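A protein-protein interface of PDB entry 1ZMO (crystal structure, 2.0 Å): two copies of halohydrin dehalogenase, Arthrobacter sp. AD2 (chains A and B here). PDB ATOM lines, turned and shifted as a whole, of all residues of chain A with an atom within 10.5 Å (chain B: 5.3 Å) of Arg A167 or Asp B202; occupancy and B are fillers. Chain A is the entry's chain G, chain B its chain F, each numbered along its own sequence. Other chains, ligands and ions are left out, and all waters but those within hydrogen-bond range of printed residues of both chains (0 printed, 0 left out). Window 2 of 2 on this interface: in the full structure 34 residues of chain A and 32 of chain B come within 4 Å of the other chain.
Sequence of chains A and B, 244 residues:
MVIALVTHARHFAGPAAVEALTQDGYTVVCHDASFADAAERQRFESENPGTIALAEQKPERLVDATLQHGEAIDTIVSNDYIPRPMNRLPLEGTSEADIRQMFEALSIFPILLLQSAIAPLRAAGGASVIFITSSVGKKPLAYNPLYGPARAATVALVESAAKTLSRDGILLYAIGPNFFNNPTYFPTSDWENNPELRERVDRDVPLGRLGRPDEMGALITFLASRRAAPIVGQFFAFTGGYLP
Arg A167 touches five residues of chain B. Asp B202 touches one residue of chain A. No residue of chain A comes within 4 Å of Arg B200. No residue of chain A comes within 4 Å of Val B201. Val B205 touches just one residue of chain A: Arg A167 (2.8 Å). Gly B208 touches just one residue of chain A: Arg A167. Of the printed residues of chain A, Leu B207 touches Ser A166 (3.9 Å) and Arg A167 (3.8 Å). Of the printed residues of chain B, Lys A163 touches Pro B206. Printed residues of chain B within 4 Å of Ser A166: Pro B206 and Leu B207. Of the printed residues of chain B, Ala A162 touches Pro B206. Thr A164 touches none of the printed residues of chain B. The nearest residue of chain B that does not touch Arg A167 is Val B201 (4.1 Å). The nearest printed residue of chain B that does not touch Ala A162 is Leu B207 (5.9 Å).
Among the printed residues, merely in contact across the chains: Ala A162 with Pro B206 (3.7 Å), Lys A163 with Pro B206 (3.5 Å), Ser A166 with Pro B206 (3.8 Å), Ser A166 with Leu B207 (3.9 Å) and Arg A167 with Leu B207 (3.8 Å).
Hydrophobic or aromatic side chains of chain B within 4 Å of the printed part of chain A: Pro B206. Along chain A the printed residues that touch a printed residue of chain B span positions 162 to 167. Among the printed residues, 9 pairs touch across the chains. Among the printed residues, Asp or Glu carboxylates within 4 Å of a Lys or Arg side-chain nitrogen of the other chain: Arg A167 with Asp B202.
The guanidinium group (NH1) of Arg A167 is in hydrogen-bond range of the backbone carbonyl oxygen (O) of Val B205 (2.8 Å). The backbone NH (N) of Gly B208 sits close to the guanidinium group (NH1) of Arg A167. O of Pro B206 is in hydrogen-bond range of NH1 of Arg A167 (2.5 Å). NH2 of Arg A167 is in salt-bridge range of OD2 of Asp B202, at 3.2 Å.
OG of Ser A166 lies within hydrogen-bond range of O of Ala A162, at 2.8 Å.
No position is printed for both chains. Of the 9 pairs that touch across the chains among the printed residues, none has its exchanged pair printed and touching as well.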
ATOM      1  N   ILE A 118     -14.276 -15.227 -24.082  1.00  0.00           N
ATOM      2  CA  ILE A 118     -14.368 -16.659 -23.883  1.00  0.00           C
ATOM      3  C   ILE A 118     -13.431 -17.517 -24.780  1.00  0.00           C
ATOM      4  O   ILE A 118     -12.518 -18.199 -24.271  1.00  0.00           O
ATOM      5  CB  ILE A 118     -15.866 -17.139 -23.952  1.00  0.00           C
ATOM      6  CG1 ILE A 118     -16.694 -16.485 -22.807  1.00  0.00           C
ATOM      7  CG2 ILE A 118     -15.932 -18.665 -23.713  1.00  0.00           C
ATOM      8  CD1 ILE A 118     -18.211 -16.505 -23.020  1.00  0.00           C
ATOM      9  N   LEU A 121      -9.646 -17.064 -23.941  1.00  0.00           N
ATOM     10  CA  LEU A 121      -9.246 -17.391 -22.575  1.00  0.00           C
ATOM     11  C   LEU A 121      -9.371 -18.907 -22.427  1.00  0.00           C
ATOM     12  O   LEU A 121      -8.637 -19.538 -21.639  1.00  0.00           O
ATOM     13  CB  LEU A 121     -10.120 -16.623 -21.554  1.00  0.00           C
ATOM     14  CG  LEU A 121      -9.639 -15.261 -21.007  1.00  0.00           C
ATOM     15  CD1 LEU A 121      -9.057 -14.353 -22.074  1.00  0.00           C
ATOM     16  CD2 LEU A 121     -10.829 -14.583 -20.311  1.00  0.00           C
ATOM     17  N   ARG A 122     -10.261 -19.497 -23.224  1.00  0.00           N
ATOM     18  CA  ARG A 122     -10.453 -20.954 -23.178  1.00  0.00           C
ATOM     19  C   ARG A 122      -9.302 -21.657 -23.862  1.00  0.00           C
ATOM     20  O   ARG A 122      -8.751 -22.638 -23.371  1.00  0.00           O
ATOM     21  CB  ARG A 122     -11.742 -21.368 -23.874  1.00  0.00           C
ATOM     22  CG  ARG A 122     -11.946 -22.867 -23.924  1.00  0.00           C
ATOM     23  CD  ARG A 122     -13.425 -23.199 -24.061  1.00  0.00           C
ATOM     24  NE  ARG A 122     -14.001 -22.540 -25.210  1.00  0.00           N
ATOM     25  CZ  ARG A 122     -15.261 -22.124 -25.270  1.00  0.00           C
ATOM     26  NH1 ARG A 122     -15.690 -21.545 -26.371  1.00  0.00           N
ATOM     27  NH2 ARG A 122     -16.079 -22.264 -24.221  1.00  0.00           N
ATOM     28  N   ALA A 123      -8.962 -21.151 -25.024  1.00  0.00           N
ATOM     29  CA  ALA A 123      -7.875 -21.735 -25.776  1.00  0.00           C
ATOM     30  C   ALA A 123      -6.535 -21.628 -25.009  1.00  0.00           C
ATOM     31  O   ALA A 123      -5.645 -22.455 -25.184  1.00  0.00           O
ATOM     32  CB  ALA A 123      -7.804 -21.063 -27.150  1.00  0.00           C
ATOM     33  N   GLY A 125      -6.412 -21.944 -21.925  1.00  0.00           N
ATOM     34  CA  GLY A 125      -6.567 -22.909 -20.878  1.00  0.00           C
ATOM     35  C   GLY A 125      -7.023 -22.262 -19.601  1.00  0.00           C
ATOM     36  O   GLY A 125      -6.741 -22.813 -18.517  1.00  0.00           O
ATOM     37  N   GLY A 126      -7.700 -21.114 -19.719  1.00  0.00           N
ATOM     38  CA  GLY A 126      -8.202 -20.405 -18.550  1.00  0.00           C
ATOM     39  C   GLY A 126      -7.620 -19.044 -18.177  1.00  0.00           C
ATOM     40  O   GLY A 126      -6.642 -18.514 -18.758  1.00  0.00           O
ATOM     41  N   ALA A 127      -8.245 -18.462 -17.158  1.00  0.00           N
ATOM     42  CA  ALA A 127      -7.869 -17.144 -16.645  1.00  0.00           C
ATOM     43  C   ALA A 127      -8.920 -16.735 -15.631  1.00  0.00           C
ATOM     44  O   ALA A 127      -9.894 -17.472 -15.397  1.00  0.00           O
ATOM     45  CB  ALA A 127      -7.864 -16.114 -17.807  1.00  0.00           C
ATOM     46  N   SER A 160     -24.382 -16.739 -13.327  1.00  0.00           N
ATOM     47  CA  SER A 160     -24.877 -17.668 -14.309  1.00  0.00           C
ATOM     48  C   SER A 160     -23.745 -18.148 -15.197  1.00  0.00           C
ATOM     49  O   SER A 160     -23.517 -19.362 -15.357  1.00  0.00           O
ATOM     50  CB  SER A 160     -25.958 -17.020 -15.179  1.00  0.00           C
ATOM     51  OG  SER A 160     -26.298 -17.904 -16.203  1.00  0.00           O
ATOM     52  N   ALA A 161     -23.040 -17.191 -15.775  1.00  0.00           N
ATOM     53  CA  ALA A 161     -21.995 -17.554 -16.686  1.00  0.00           C
ATOM     54  C   ALA A 161     -20.998 -18.498 -16.042  1.00  0.00           C
ATOM     55  O   ALA A 161     -20.511 -19.379 -16.696  1.00  0.00           O
ATOM     56  CB  ALA A 161     -21.327 -16.337 -17.194  1.00  0.00           C
ATOM     57  N   ALA A 162     -20.715 -18.344 -14.753  1.00  0.00           N
ATOM     58  CA  ALA A 162     -19.743 -19.200 -14.087  1.00  0.00           C
ATOM     59  C   ALA A 162     -20.054 -20.689 -14.126  1.00  0.00           C
ATOM     60  O   ALA A 162     -19.130 -21.515 -14.158  1.00  0.00           O
ATOM     61  CB  ALA A 162     -19.555 -18.770 -12.630  1.00  0.00           C
ATOM     62  N   LYS A 163     -21.346 -21.019 -14.107  1.00  0.00           N
ATOM     63  CA  LYS A 163     -21.804 -22.413 -14.095  1.00  0.00           C
ATOM     64  C   LYS A 163     -21.249 -23.228 -15.271  1.00  0.00           C
ATOM     65  O   LYS A 163     -21.139 -24.451 -15.170  1.00  0.00           O
ATOM     66  CB  LYS A 163     -23.338 -22.459 -14.118  1.00  0.00           C
ATOM     67  CG  LYS A 163     -24.014 -21.681 -12.992  1.00  0.00           C
ATOM     68  CD  LYS A 163     -23.343 -21.908 -11.606  1.00  0.00           C
ATOM     69  CE  LYS A 163     -24.414 -21.593 -10.535  1.00  0.00           C
ATOM     70  NZ  LYS A 163     -23.749 -21.243  -9.298  1.00  0.00           N
ATOM     71  N   THR A 164     -20.909 -22.557 -16.371  1.00  0.00           N
ATOM     72  CA  THR A 164     -20.378 -23.239 -17.519  1.00  0.00           C
ATOM     73  C   THR A 164     -18.896 -22.856 -17.741  1.00  0.00           C
ATOM     74  O   THR A 164     -18.063 -23.714 -18.022  1.00  0.00           O
ATOM     75  CB  THR A 164     -21.229 -22.933 -18.804  1.00  0.00           C
ATOM     76  OG1 THR A 164     -21.248 -21.526 -19.033  1.00  0.00           O
ATOM     77  CG2 THR A 164     -22.739 -23.382 -18.619  1.00  0.00           C
ATOM     78  N   LEU A 165     -18.540 -21.589 -17.580  1.00  0.00           N
ATOM     79  CA  LEU A 165     -17.168 -21.203 -17.830  1.00  0.00           C
ATOM     80  C   LEU A 165     -16.103 -21.808 -16.904  1.00  0.00           C
ATOM     81  O   LEU A 165     -14.956 -22.079 -17.355  1.00  0.00           O
ATOM     82  CB  LEU A 165     -17.048 -19.673 -17.866  1.00  0.00           C
ATOM     83  CG  LEU A 165     -17.956 -19.035 -18.937  1.00  0.00           C
ATOM     84  CD1 LEU A 165     -17.756 -17.563 -18.890  1.00  0.00           C
ATOM     85  CD2 LEU A 165     -17.627 -19.557 -20.352  1.00  0.00           C
ATOM     86  N   SER A 166     -16.467 -22.045 -15.646  1.00  0.00           N
ATOM     87  CA  SER A 166     -15.505 -22.609 -14.677  1.00  0.00           C
ATOM     88  C   SER A 166     -14.890 -23.919 -15.205  1.00  0.00           C
ATOM     89  O   SER A 166     -13.714 -24.237 -14.946  1.00  0.00           O
ATOM     90  CB  SER A 166     -16.181 -22.880 -13.342  1.00  0.00           C
ATOM     91  OG  SER A 166     -16.722 -21.711 -12.762  1.00  0.00           O
ATOM     92  N   ARG A 167     -15.692 -24.674 -15.933  1.00  0.00           N
ATOM     93  CA  ARG A 167     -15.225 -25.920 -16.523  1.00  0.00           C
ATOM     94  C   ARG A 167     -14.048 -25.711 -17.458  1.00  0.00           C
ATOM     95  O   ARG A 167     -13.258 -26.620 -17.623  1.00  0.00           O
ATOM     96  CB  ARG A 167     -16.323 -26.594 -17.337  1.00  0.00           C
ATOM     97  CG  ARG A 167     -16.992 -27.763 -16.665  1.00  0.00           C
ATOM     98  CD  ARG A 167     -16.156 -29.064 -16.671  1.00  0.00           C
ATOM     99  NE  ARG A 167     -17.000 -30.183 -16.211  1.00  0.00           N
ATOM    100  CZ  ARG A 167     -17.604 -30.188 -15.034  1.00  0.00           C
ATOM    101  NH1 ARG A 167     -17.435 -29.156 -14.233  1.00  0.00           N
ATOM    102  NH2 ARG A 167     -18.397 -31.185 -14.670  1.00  0.00           N
ATOM    103  N   ASP A 168     -13.969 -24.550 -18.100  1.00  0.00           N
ATOM    104  CA  ASP A 168     -12.881 -24.248 -19.052  1.00  0.00           C
ATOM    105  C   ASP A 168     -11.741 -23.589 -18.326  1.00  0.00           C
ATOM    106  O   ASP A 168     -10.762 -23.227 -18.939  1.00  0.00           O
ATOM    107  CB  ASP A 168     -13.345 -23.275 -20.152  1.00  0.00           C
ATOM    108  CG  ASP A 168     -14.261 -23.926 -21.173  1.00  0.00           C
ATOM    109  OD1 ASP A 168     -13.973 -25.067 -21.580  1.00  0.00           O
ATOM    110  OD2 ASP A 168     -15.269 -23.295 -21.589  1.00  0.00           O
ATOM    111  N   GLY A 169     -11.874 -23.438 -17.006  1.00  0.00           N
ATOM    112  CA  GLY A 169     -10.847 -22.778 -16.222  1.00  0.00           C
ATOM    113  C   GLY A 169     -11.008 -21.246 -16.243  1.00  0.00           C
ATOM    114  O   GLY A 169     -10.111 -20.511 -15.802  1.00  0.00           O
ATOM    115  N   ILE A 170     -12.152 -20.764 -16.749  1.00  0.00           N
ATOM    116  CA  ILE A 170     -12.381 -19.329 -16.782  1.00  0.00           C
ATOM    117  C   ILE A 170     -13.227 -19.022 -15.553  1.00  0.00           C
ATOM    118  O   ILE A 170     -14.435 -19.304 -15.514  1.00  0.00           O
ATOM    119  CB  ILE A 170     -13.057 -18.889 -18.111  1.00  0.00           C
ATOM    120  CG1 ILE A 170     -12.203 -19.374 -19.314  1.00  0.00           C
ATOM    121  CG2 ILE A 170     -13.160 -17.318 -18.135  1.00  0.00           C
ATOM    122  CD1 ILE A 170     -12.989 -19.627 -20.642  1.00  0.00           C
ATOM    123  N   LEU A 171     -12.557 -18.457 -14.546  1.00  0.00           N
ATOM    124  CA  LEU A 171     -13.130 -18.156 -13.222  1.00  0.00           C
ATOM    125  C   LEU A 171     -13.618 -16.725 -13.118  1.00  0.00           C
ATOM    126  O   LEU A 171     -12.821 -15.766 -13.186  1.00  0.00           O
ATOM    127  CB  LEU A 171     -12.070 -18.453 -12.163  1.00  0.00           C
ATOM    128  CG  LEU A 171     -11.357 -19.799 -12.461  1.00  0.00           C
ATOM    129  CD1 LEU A 171     -10.118 -20.016 -11.494  1.00  0.00           C
ATOM    130  CD2 LEU A 171     -12.364 -20.951 -12.345  1.00  0.00           C
ATOM    131  N   LEU A 172     -14.946 -16.604 -12.996  1.00  0.00           N
ATOM    132  CA  LEU A 172     -15.626 -15.306 -12.902  1.00  0.00           C
ATOM    133  C   LEU A 172     -15.919 -14.929 -11.460  1.00  0.00           C
ATOM    134  O   LEU A 172     -16.191 -15.796 -10.662  1.00  0.00           O
ATOM    135  CB  LEU A 172     -16.963 -15.354 -13.649  1.00  0.00           C
ATOM    136  CG  LEU A 172     -16.889 -15.054 -15.156  1.00  0.00           C
ATOM    137  CD1 LEU A 172     -15.684 -15.777 -15.781  1.00  0.00           C
ATOM    138  CD2 LEU A 172     -18.252 -15.350 -15.844  1.00  0.00           C
ATOM    139  N   ARG A 226      -5.687 -17.263  -8.496  1.00  0.00           N
ATOM    140  CA  ARG A 226      -6.391 -18.537  -8.646  1.00  0.00           C
ATOM    141  C   ARG A 226      -5.998 -19.561  -7.567  1.00  0.00           C
ATOM    142  O   ARG A 226      -6.330 -20.735  -7.709  1.00  0.00           O
ATOM    143  CB  ARG A 226      -6.152 -19.249 -10.007  1.00  0.00           C
ATOM    144  CG  ARG A 226      -6.512 -18.435 -11.249  1.00  0.00           C
ATOM    145  CD  ARG A 226      -6.240 -19.276 -12.491  1.00  0.00           C
ATOM    146  NE  ARG A 226      -5.672 -18.463 -13.562  1.00  0.00           N
ATOM    147  CZ  ARG A 226      -5.442 -18.911 -14.798  1.00  0.00           C
ATOM    148  NH1 ARG A 226      -5.723 -20.178 -15.119  1.00  0.00           N
ATOM    149  NH2 ARG A 226      -4.936 -18.079 -15.721  1.00  0.00           N
ATOM    150  N   ALA A 229      -9.510 -21.182  -6.199  1.00  0.00           N
ATOM    151  CA  ALA A 229     -10.486 -21.330  -7.292  1.00  0.00           C
ATOM    152  C   ALA A 229     -11.888 -21.768  -6.865  1.00  0.00           C
ATOM    153  O   ALA A 229     -12.863 -21.341  -7.476  1.00  0.00           O
ATOM    154  CB  ALA A 229      -9.940 -22.301  -8.401  1.00  0.00           C
ATOM    155  N   VAL A 232     -15.112 -19.555  -6.848  1.00  0.00           N
ATOM    156  CA  VAL A 232     -15.498 -19.048  -8.123  1.00  0.00           C
ATOM    157  C   VAL A 232     -17.034 -18.792  -8.221  1.00  0.00           C
ATOM    158  O   VAL A 232     -17.830 -19.454  -7.529  1.00  0.00           O
ATOM    159  CB  VAL A 232     -15.028 -20.068  -9.232  1.00  0.00           C
ATOM    160  CG1 VAL A 232     -15.547 -21.554  -8.936  1.00  0.00           C
ATOM    161  CG2 VAL A 232     -15.495 -19.590 -10.611  1.00  0.00           C
ATOM    162  N   GLY A 233     -17.435 -17.825  -9.055  1.00  0.00           N
ATOM    163  CA  GLY A 233     -18.873 -17.587  -9.317  1.00  0.00           C
ATOM    164  C   GLY A 233     -19.709 -16.835  -8.318  1.00  0.00           C
ATOM    165  O   GLY A 233     -20.931 -16.838  -8.406  1.00  0.00           O
ATOM    166  N   LEU B 197     -19.791 -40.572  -6.691  1.00  0.00           N
ATOM    167  CA  LEU B 197     -19.457 -39.230  -6.231  1.00  0.00           C
ATOM    168  C   LEU B 197     -18.777 -38.514  -7.383  1.00  0.00           C
ATOM    169  O   LEU B 197     -18.950 -37.304  -7.564  1.00  0.00           O
ATOM    170  CB  LEU B 197     -18.530 -39.254  -5.006  1.00  0.00           C
ATOM    171  CG  LEU B 197     -17.872 -37.908  -4.611  1.00  0.00           C
ATOM    172  CD1 LEU B 197     -18.923 -36.892  -4.124  1.00  0.00           C
ATOM    173  CD2 LEU B 197     -16.804 -38.163  -3.527  1.00  0.00           C
ATOM    174  N   ARG B 198     -18.007 -39.263  -8.162  1.00  0.00           N
ATOM    175  CA  ARG B 198     -17.328 -38.700  -9.326  1.00  0.00           C
ATOM    176  C   ARG B 198     -18.346 -38.089 -10.284  1.00  0.00           C
ATOM    177  O   ARG B 198     -18.160 -36.976 -10.750  1.00  0.00           O
ATOM    178  CB  ARG B 198     -16.590 -39.785 -10.075  1.00  0.00           C
ATOM    179  CG  ARG B 198     -15.146 -39.572 -10.197  1.00  0.00           C
ATOM    180  CD  ARG B 198     -14.481 -39.966  -8.934  1.00  0.00           C
ATOM    181  NE  ARG B 198     -13.212 -40.612  -9.210  1.00  0.00           N
ATOM    182  CZ  ARG B 198     -13.084 -41.783  -9.830  1.00  0.00           C
ATOM    183  NH1 ARG B 198     -11.869 -42.293 -10.034  1.00  0.00           N
ATOM    184  NH2 ARG B 198     -14.162 -42.446 -10.242  1.00  0.00           N
ATOM    185  N   GLU B 199     -19.416 -38.837 -10.578  1.00  0.00           N
ATOM    186  CA  GLU B 199     -20.477 -38.397 -11.499  1.00  0.00           C
ATOM    187  C   GLU B 199     -21.328 -37.258 -10.991  1.00  0.00           C
ATOM    188  O   GLU B 199     -21.776 -36.428 -11.784  1.00  0.00           O
ATOM    189  CB  GLU B 199     -21.384 -39.577 -11.867  1.00  0.00           C
ATOM    190  N   ARG B 200     -21.594 -37.216  -9.683  1.00  0.00           N
ATOM    191  CA  ARG B 200     -22.384 -36.108  -9.140  1.00  0.00           C
ATOM    192  C   ARG B 200     -21.564 -34.832  -9.347  1.00  0.00           C
ATOM    193  O   ARG B 200     -22.058 -33.860  -9.889  1.00  0.00           O
ATOM    194  CB  ARG B 200     -22.664 -36.296  -7.638  1.00  0.00           C
ATOM    195  N   VAL B 201     -20.304 -34.859  -8.912  1.00  0.00           N
ATOM    196  CA  VAL B 201     -19.412 -33.714  -9.052  1.00  0.00           C
ATOM    197  C   VAL B 201     -19.346 -33.230 -10.516  1.00  0.00           C
ATOM    198  O   VAL B 201     -19.355 -32.027 -10.793  1.00  0.00           O
ATOM    199  CB  VAL B 201     -18.007 -34.078  -8.459  1.00  0.00           C
ATOM    200  CG1 VAL B 201     -16.998 -32.968  -8.725  1.00  0.00           C
ATOM    201  CG2 VAL B 201     -18.145 -34.290  -6.954  1.00  0.00           C
ATOM    202  N   ASP B 202     -19.303 -34.167 -11.452  1.00  0.00           N
ATOM    203  CA  ASP B 202     -19.286 -33.837 -12.867  1.00  0.00           C
ATOM    204  C   ASP B 202     -20.551 -33.015 -13.150  1.00  0.00           C
ATOM    205  O   ASP B 202     -20.518 -31.937 -13.687  1.00  0.00           O
ATOM    206  CB  ASP B 202     -19.332 -35.119 -13.686  1.00  0.00           C
ATOM    207  CG  ASP B 202     -19.197 -34.854 -15.177  1.00  0.00           C
ATOM    208  OD1 ASP B 202     -20.080 -35.301 -15.933  1.00  0.00           O
ATOM    209  OD2 ASP B 202     -18.213 -34.199 -15.600  1.00  0.00           O
ATOM    210  N   ARG B 203     -21.664 -33.575 -12.742  1.00  0.00           N
ATOM    211  CA  ARG B 203     -22.969 -33.003 -12.891  1.00  0.00           C
ATOM    212  C   ARG B 203     -23.246 -31.680 -12.169  1.00  0.00           C
ATOM    213  O   ARG B 203     -23.822 -30.767 -12.751  1.00  0.00           O
ATOM    214  CB  ARG B 203     -23.986 -34.035 -12.420  1.00  0.00           C
ATOM    215  CG  ARG B 203     -25.405 -33.494 -12.279  1.00  0.00           C
ATOM    216  CD  ARG B 203     -26.312 -34.445 -11.467  1.00  0.00           C
ATOM    217  NE  ARG B 203     -26.236 -35.789 -12.004  1.00  0.00           N
ATOM    218  CZ  ARG B 203     -25.738 -36.832 -11.348  1.00  0.00           C
ATOM    219  NH1 ARG B 203     -25.276 -36.689 -10.114  1.00  0.00           N
ATOM    220  NH2 ARG B 203     -25.689 -38.019 -11.938  1.00  0.00           N
ATOM    221  N   ASP B 204     -22.850 -31.550 -10.913  1.00  0.00           N
ATOM    222  CA  ASP B 204     -23.212 -30.349 -10.169  1.00  0.00           C
ATOM    223  C   ASP B 204     -22.180 -29.343  -9.780  1.00  0.00           C
ATOM    224  O   ASP B 204     -22.543 -28.348  -9.152  1.00  0.00           O
ATOM    225  CB  ASP B 204     -23.905 -30.733  -8.879  1.00  0.00           C
ATOM    226  CG  ASP B 204     -25.098 -31.600  -9.093  1.00  0.00           C
ATOM    227  OD1 ASP B 204     -25.852 -31.345 -10.050  1.00  0.00           O
ATOM    228  OD2 ASP B 204     -25.295 -32.526  -8.277  1.00  0.00           O
ATOM    229  N   VAL B 205     -20.902 -29.605 -10.080  1.00  0.00           N
ATOM    230  CA  VAL B 205     -19.858 -28.674  -9.703  1.00  0.00           C
ATOM    231  C   VAL B 205     -19.204 -28.055 -10.945  1.00  0.00           C
ATOM    232  O   VAL B 205     -18.385 -28.671 -11.594  1.00  0.00           O
ATOM    233  CB  VAL B 205     -18.720 -29.351  -8.879  1.00  0.00           C
ATOM    234  CG1 VAL B 205     -17.614 -28.308  -8.546  1.00  0.00           C
ATOM    235  CG2 VAL B 205     -19.231 -29.948  -7.683  1.00  0.00           C
ATOM    236  N   PRO B 206     -19.537 -26.801 -11.255  1.00  0.00           N
ATOM    237  CA  PRO B 206     -18.944 -26.166 -12.436  1.00  0.00           C
ATOM    238  C   PRO B 206     -17.442 -26.410 -12.546  1.00  0.00           C
ATOM    239  O   PRO B 206     -16.951 -26.768 -13.612  1.00  0.00           O
ATOM    240  CB  PRO B 206     -19.307 -24.693 -12.255  1.00  0.00           C
ATOM    241  CG  PRO B 206     -20.715 -24.792 -11.636  1.00  0.00           C
ATOM    242  CD  PRO B 206     -20.529 -25.933 -10.601  1.00  0.00           C
ATOM    243  N   LEU B 207     -16.724 -26.197 -11.454  1.00  0.00           N
ATOM    244  CA  LEU B 207     -15.265 -26.405 -11.393  1.00  0.00           C
ATOM    245  C   LEU B 207     -14.884 -27.878 -11.783  1.00  0.00           C
ATOM    246  O   LEU B 207     -13.742 -28.169 -12.116  1.00  0.00           O
ATOM    247  CB  LEU B 207     -14.746 -26.083  -9.970  1.00  0.00           C
ATOM    248  CG  LEU B 207     -13.546 -25.145  -9.694  1.00  0.00           C
ATOM    249  CD1 LEU B 207     -12.546 -25.831  -8.796  1.00  0.00           C
ATOM    250  CD2 LEU B 207     -12.849 -24.721 -10.947  1.00  0.00           C
ATOM    251  N   GLY B 208     -15.844 -28.793 -11.704  1.00  0.00           N
ATOM    252  CA  GLY B 208     -15.635 -30.176 -12.114  1.00  0.00           C
ATOM    253  C   GLY B 208     -14.753 -31.043 -11.261  1.00  0.00           C
ATOM    254  O   GLY B 208     -14.289 -32.091 -11.726  1.00  0.00           O
